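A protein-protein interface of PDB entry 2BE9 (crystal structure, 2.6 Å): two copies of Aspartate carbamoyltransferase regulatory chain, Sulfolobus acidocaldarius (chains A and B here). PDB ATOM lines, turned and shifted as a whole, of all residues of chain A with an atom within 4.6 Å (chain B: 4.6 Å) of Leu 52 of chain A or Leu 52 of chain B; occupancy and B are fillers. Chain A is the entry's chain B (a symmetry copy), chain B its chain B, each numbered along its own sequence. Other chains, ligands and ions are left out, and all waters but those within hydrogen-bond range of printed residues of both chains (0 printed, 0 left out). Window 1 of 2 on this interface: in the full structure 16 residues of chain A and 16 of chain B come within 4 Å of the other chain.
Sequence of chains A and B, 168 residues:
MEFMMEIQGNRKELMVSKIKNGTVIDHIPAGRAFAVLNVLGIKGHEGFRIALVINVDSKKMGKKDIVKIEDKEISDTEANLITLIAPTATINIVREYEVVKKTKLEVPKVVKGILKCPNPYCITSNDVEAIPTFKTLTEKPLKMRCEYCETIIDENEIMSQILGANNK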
ATOM      1  N   ALA A  33      13.846   9.969  36.079  1.00  0.00           N
ATOM      2  CA  ALA A  33      13.280  10.484  34.843  1.00  0.00           C
ATOM      3  C   ALA A  33      13.550   9.557  33.669  1.00  0.00           C
ATOM      4  O   ALA A  33      12.643   9.318  32.846  1.00  0.00           O
ATOM      5  CB  ALA A  33      13.791  11.857  34.545  1.00  0.00           C
ATOM      6  N   PHE A  34      14.774   9.020  33.604  1.00  0.00           N
ATOM      7  CA  PHE A  34      15.159   8.145  32.506  1.00  0.00           C
ATOM      8  C   PHE A  34      14.259   6.943  32.474  1.00  0.00           C
ATOM      9  O   PHE A  34      13.855   6.507  31.389  1.00  0.00           O
ATOM     10  CB  PHE A  34      16.627   7.704  32.572  1.00  0.00           C
ATOM     11  CG  PHE A  34      17.597   8.840  32.484  1.00  0.00           C
ATOM     12  CD1 PHE A  34      18.350   9.218  33.606  1.00  0.00           C
ATOM     13  CD2 PHE A  34      17.743   9.561  31.293  1.00  0.00           C
ATOM     14  CE1 PHE A  34      19.255  10.303  33.539  1.00  0.00           C
ATOM     15  CE2 PHE A  34      18.626  10.656  31.216  1.00  0.00           C
ATOM     16  CZ  PHE A  34      19.388  11.024  32.337  1.00  0.00           C
ATOM     17  N   LEU A  37      10.665   7.854  30.973  1.00  0.00           N
ATOM     18  CA  LEU A  37      10.726   7.811  29.507  1.00  0.00           C
ATOM     19  C   LEU A  37      10.694   6.389  28.950  1.00  0.00           C
ATOM     20  O   LEU A  37       9.954   6.123  28.006  1.00  0.00           O
ATOM     21  CB  LEU A  37      11.991   8.519  29.009  1.00  0.00           C
ATOM     22  CG  LEU A  37      11.983   9.968  28.499  1.00  0.00           C
ATOM     23  CD1 LEU A  37      10.817  10.784  29.013  1.00  0.00           C
ATOM     24  CD2 LEU A  37      13.295  10.645  28.840  1.00  0.00           C
ATOM     25  N   ILE A  50      12.003  17.100  23.858  1.00  0.00           N
ATOM     26  CA  ILE A  50      11.914  16.623  25.232  1.00  0.00           C
ATOM     27  C   ILE A  50      12.897  17.391  26.103  1.00  0.00           C
ATOM     28  O   ILE A  50      14.015  17.673  25.694  1.00  0.00           O
ATOM     29  CB  ILE A  50      12.210  15.102  25.343  1.00  0.00           C
ATOM     30  CG1 ILE A  50      11.192  14.268  24.561  1.00  0.00           C
ATOM     31  CG2 ILE A  50      12.220  14.639  26.802  1.00  0.00           C
ATOM     32  CD1 ILE A  50      11.758  12.935  24.107  1.00  0.00           C
ATOM     33  N   ALA A  51      12.467  17.740  27.306  1.00  0.00           N
ATOM     34  CA  ALA A  51      13.365  18.300  28.294  1.00  0.00           C
ATOM     35  C   ALA A  51      13.297  17.491  29.584  1.00  0.00           C
ATOM     36  O   ALA A  51      12.208  17.077  30.007  1.00  0.00           O
ATOM     37  CB  ALA A  51      13.043  19.739  28.563  1.00  0.00           C
ATOM     38  N   LEU A  52      14.466  17.239  30.180  1.00  0.00           N
ATOM     39  CA  LEU A  52      14.532  16.728  31.528  1.00  0.00           C
ATOM     40  C   LEU A  52      15.444  17.593  32.386  1.00  0.00           C
ATOM     41  O   LEU A  52      16.452  18.122  31.915  1.00  0.00           O
ATOM     42  CB  LEU A  52      15.058  15.304  31.590  1.00  0.00           C
ATOM     43  CG  LEU A  52      15.386  14.327  30.477  1.00  0.00           C
ATOM     44  CD1 LEU A  52      15.407  12.991  31.150  1.00  0.00           C
ATOM     45  CD2 LEU A  52      14.398  14.292  29.379  1.00  0.00           C
ATOM     46  N   VAL A  53      15.072  17.733  33.654  1.00  0.00           N
ATOM     47  CA  VAL A  53      16.002  18.195  34.656  1.00  0.00           C
ATOM     48  C   VAL A  53      16.085  17.106  35.714  1.00  0.00           C
ATOM     49  O   VAL A  53      15.081  16.512  36.091  1.00  0.00           O
ATOM     50  CB  VAL A  53      15.631  19.584  35.223  1.00  0.00           C
ATOM     51  CG1 VAL A  53      15.491  20.566  34.084  1.00  0.00           C
ATOM     52  CG2 VAL A  53      14.333  19.536  35.995  1.00  0.00           C
ATOM     53  N   ILE A  54      17.291  16.823  36.177  1.00  0.00           N
ATOM     54  CA  ILE A  54      17.484  15.726  37.097  1.00  0.00           C
ATOM     55  C   ILE A  54      18.168  16.205  38.369  1.00  0.00           C
ATOM     56  O   ILE A  54      19.129  16.972  38.312  1.00  0.00           O
ATOM     57  CB  ILE A  54      18.225  14.574  36.381  1.00  0.00           C
ATOM     58  CG1 ILE A  54      17.230  13.876  35.449  1.00  0.00           C
ATOM     59  CG2 ILE A  54      18.779  13.552  37.358  1.00  0.00           C
ATOM     60  CD1 ILE A  54      17.817  13.458  34.171  1.00  0.00           C
ATOM     61  N   ILE A  66      12.046  16.410  36.643  1.00  0.00           N
ATOM     62  CA  ILE A  66      10.929  16.851  35.849  1.00  0.00           C
ATOM     63  C   ILE A  66      11.142  16.445  34.396  1.00  0.00           C
ATOM     64  O   ILE A  66      12.243  16.613  33.840  1.00  0.00           O
ATOM     65  CB  ILE A  66      10.758  18.377  35.884  1.00  0.00           C
ATOM     66  CG1 ILE A  66      10.643  18.906  37.320  1.00  0.00           C
ATOM     67  CG2 ILE A  66       9.546  18.805  35.049  1.00  0.00           C
ATOM     68  CD1 ILE A  66      10.975  20.418  37.434  1.00  0.00           C
ATOM     69  N   ALA B  33      21.750  12.713  22.980  1.00  0.00           N
ATOM     70  CA  ALA B  33      22.140  13.153  24.310  1.00  0.00           C
ATOM     71  C   ALA B  33      22.256  11.988  25.279  1.00  0.00           C
ATOM     72  O   ALA B  33      23.216  11.936  26.074  1.00  0.00           O
ATOM     73  CB  ALA B  33      21.186  14.174  24.843  1.00  0.00           C
ATOM     74  N   PHE B  34      21.305  11.050  25.200  1.00  0.00           N
ATOM     75  CA  PHE B  34      21.293   9.906  26.100  1.00  0.00           C
ATOM     76  C   PHE B  34      22.560   9.118  25.938  1.00  0.00           C
ATOM     77  O   PHE B  34      23.131   8.657  26.934  1.00  0.00           O
ATOM     78  CB  PHE B  34      20.075   8.995  25.902  1.00  0.00           C
ATOM     79  CG  PHE B  34      18.769   9.675  26.168  1.00  0.00           C
ATOM     80  CD1 PHE B  34      17.892   9.965  25.111  1.00  0.00           C
ATOM     81  CD2 PHE B  34      18.418  10.062  27.467  1.00  0.00           C
ATOM     82  CE1 PHE B  34      16.664  10.626  25.350  1.00  0.00           C
ATOM     83  CE2 PHE B  34      17.208  10.736  27.717  1.00  0.00           C
ATOM     84  CZ  PHE B  34      16.326  11.015  26.659  1.00  0.00           C
ATOM     85  N   LEU B  37      25.649  10.943  27.706  1.00  0.00           N
ATOM     86  CA  LEU B  37      25.657  10.607  29.135  1.00  0.00           C
ATOM     87  C   LEU B  37      26.211   9.211  29.415  1.00  0.00           C
ATOM     88  O   LEU B  37      27.029   9.052  30.318  1.00  0.00           O
ATOM     89  CB  LEU B  37      24.242  10.715  29.714  1.00  0.00           C
ATOM     90  CG  LEU B  37      23.754  11.949  30.486  1.00  0.00           C
ATOM     91  CD1 LEU B  37      24.537  13.206  30.174  1.00  0.00           C
ATOM     92  CD2 LEU B  37      22.276  12.169  30.233  1.00  0.00           C
ATOM     93  N   ILE B  50      21.371  17.605  36.378  1.00  0.00           N
ATOM     94  CA  ILE B  50      21.575  17.458  34.944  1.00  0.00           C
ATOM     95  C   ILE B  50      20.355  17.977  34.199  1.00  0.00           C
ATOM     96  O   ILE B  50      19.224  17.763  34.615  1.00  0.00           O
ATOM     97  CB  ILE B  50      21.833  15.980  34.539  1.00  0.00           C
ATOM     98  CG1 ILE B  50      23.107  15.430  35.186  1.00  0.00           C
ATOM     99  CG2 ILE B  50      21.937  15.826  33.020  1.00  0.00           C
ATOM    100  CD1 ILE B  50      23.066  13.922  35.361  1.00  0.00           C
ATOM    101  N   ALA B  51      20.591  18.674  33.098  1.00  0.00           N
ATOM    102  CA  ALA B  51      19.519  19.055  32.202  1.00  0.00           C
ATOM    103  C   ALA B  51      19.824  18.580  30.787  1.00  0.00           C
ATOM    104  O   ALA B  51      20.974  18.665  30.332  1.00  0.00           O
ATOM    105  CB  ALA B  51      19.301  20.538  32.220  1.00  0.00           C
ATOM    106  N   LEU B  52      18.800  18.046  30.114  1.00  0.00           N
ATOM    107  CA  LEU B  52      18.873  17.807  28.692  1.00  0.00           C
ATOM    108  C   LEU B  52      17.684  18.438  27.981  1.00  0.00           C
ATOM    109  O   LEU B  52      16.572  18.478  28.508  1.00  0.00           O
ATOM    110  CB  LEU B  52      18.884  16.329  28.346  1.00  0.00           C
ATOM    111  CG  LEU B  52      18.961  15.109  29.244  1.00  0.00           C
ATOM    112  CD1 LEU B  52      19.391  14.003  28.333  1.00  0.00           C
ATOM    113  CD2 LEU B  52      19.935  15.220  30.350  1.00  0.00           C
ATOM    114  N   VAL B  53      17.939  18.937  26.776  1.00  0.00           N
ATOM    115  CA  VAL B  53      16.871  19.219  25.846  1.00  0.00           C
ATOM    116  C   VAL B  53      17.143  18.390  24.600  1.00  0.00           C
ATOM    117  O   VAL B  53      18.278  18.273  24.153  1.00  0.00           O
ATOM    118  CB  VAL B  53      16.707  20.728  25.564  1.00  0.00           C
ATOM    119  CG1 VAL B  53      16.529  21.464  26.870  1.00  0.00           C
ATOM    120  CG2 VAL B  53      17.909  21.289  24.842  1.00  0.00           C
ATOM    121  N   ILE B  54      16.099  17.790  24.052  1.00  0.00           N
ATOM    122  CA  ILE B  54      16.275  16.889  22.936  1.00  0.00           C
ATOM    123  C   ILE B  54      15.423  17.325  21.754  1.00  0.00           C
ATOM    124  O   ILE B  54      14.254  17.677  21.920  1.00  0.00           O
ATOM    125  CB  ILE B  54      16.016  15.438  23.396  1.00  0.00           C
ATOM    126  CG1 ILE B  54      17.226  14.975  24.215  1.00  0.00           C
ATOM    127  CG2 ILE B  54      15.826  14.488  22.227  1.00  0.00           C
ATOM    128  CD1 ILE B  54      16.870  14.145  25.371  1.00  0.00           C
ATOM    129  N   ILE B  66      21.131  19.357  23.699  1.00  0.00           N
ATOM    130  CA  ILE B  66      22.047  20.007  24.599  1.00  0.00           C
ATOM    131  C   ILE B  66      22.042  19.288  25.942  1.00  0.00           C
ATOM    132  O   ILE B  66      20.973  18.947  26.481  1.00  0.00           O
ATOM    133  CB  ILE B  66      21.665  21.473  24.856  1.00  0.00           C
ATOM    134  CG1 ILE B  66      21.535  22.267  23.551  1.00  0.00           C
ATOM    135  CG2 ILE B  66      22.675  22.138  25.799  1.00  0.00           C
ATOM    136  CD1 ILE B  66      20.686  23.556  23.711  1.00  0.00           C
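The backbone carbonyl oxygen of Ile 66 of chain B sits at hydrogen-bond distance from the backbone NH of Val 53 of chain B, 3.0 Å away. The backbone NH (N) of Val 53 of chain A lies within hydrogen-bond range of the backbone carbonyl oxygen (O) of Ile 66 of chain A (3.0 Å).
Among the printed residues, merely in contact across the chains: Phe 34 of chain A with Phe 34 of chain B (3.8 Å), Phe 34 of chain A with Leu 37 of chain B (3.8 Å), Leu 37 of chain A with Phe 34 of chain B (3.8 Å), Ile 50 of chain A with Leu 52 of chain B (3.9 Å), Ile 50 of chain A with Val 53 of chain B (3.3 Å), Ala 51 of chain A with Leu 52 of chain B (3.2 Å), Leu 52 of chain A with Ile 50 of chain B (3.9 Å), Leu 52 of chain A with Ala 51 of chain B (3.2 Å) and Val 53 of chain A with Ile 50 of chain B (3.3 Å).
Printed residues of chain B within 4 Å of Leu 37 of chain A: Phe 34 (3.8 Å). Of chain B, only Ile 50 (3.9 Å), Ala 51 (3.2 Å) and Leu 52 (3.0 Å) come within 4 Å of Leu 52 of chain A. Of the printed residues of chain B, Ile 54 of chain A touches Ile 50. Ile 66 of chain A touches none of the printed residues of chain B. Leu 52 of chain B touches just these residues of chain A: Ile 50, Ala 51 and Leu 52. Of the printed residues of chain A, Val 53 of chain B touches Ile 50 (3.3 Å). Of the printed residues of chain A, Ile 54 of chain B touches Ile 50. The nearest residue of chain B that does not touch Leu 52 of chain A is Phe 34 of chain B (4.5 Å). The nearest residue of chain A that does not touch Leu 52 of chain B is Phe 34 of chain A (4.5 Å). The nearest printed residue of chain A that does not touch Phe 34 of chain B is Leu 52 of chain A (4.5 Å).
Ile 50 of chain A touches Leu 52 of chain B, and with the chains exchanged Leu 52 of chain A touches Ile 50 of chain B. Ile 50 of chain A touches Val 53 of chain B, and with the chains exchanged Val 53 of chain A touches Ile 50 of chain B. Ile 50 of chain A touches Ile 54 of chain B, and with the chains exchanged Ile 54 of chain A touches Ile 50 of chain B. Ala 51 of chain A touches Leu 52 of chain B, and with the chains exchanged Leu 52 of chain A touches Ala 51 of chain B. 9 positions are printed for both chains. Of the 12 pairs that touch across the chains among the printed residues, 12 have their exchanged pair printed and touching as well.
Hydrophobic or aromatic side chains of chain B that line the printed part of chain A: Phe 34, Leu 37, Ala 51, Leu 52 and Ile 54. Printed residues of chain A that touch a printed residue of chain B: Phe 34, Leu 37, Ile 50, Ala 51, Leu 52, Val 53 and Ile 54. Hydrophobic or aromatic side chains of chain A within 4 Å of the printed part of chain B: Phe 34, Leu 37, Ala 51, Leu 52 and Ile 54. Among the printed residues, no Asp or Glu carboxylate lies within 4 Å of a Lys or Arg side-chain nitrogen of the other chain.
The backbone carbonyl oxygen of Ile 50 of chain A lies within hydrogen-bond range of the backbone NH of Ile 54 of chain B (2.7 Å). O of Ile 50 of chain B lies within hydrogen-bond range of N of Ile 54 of chain A (2.7 Å). The backbone carbonyl oxygen (O) of Leu 52 of chain B sits at hydrogen-bond distance from the backbone NH (N) of Leu 52 of chain A (3.0 Å).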
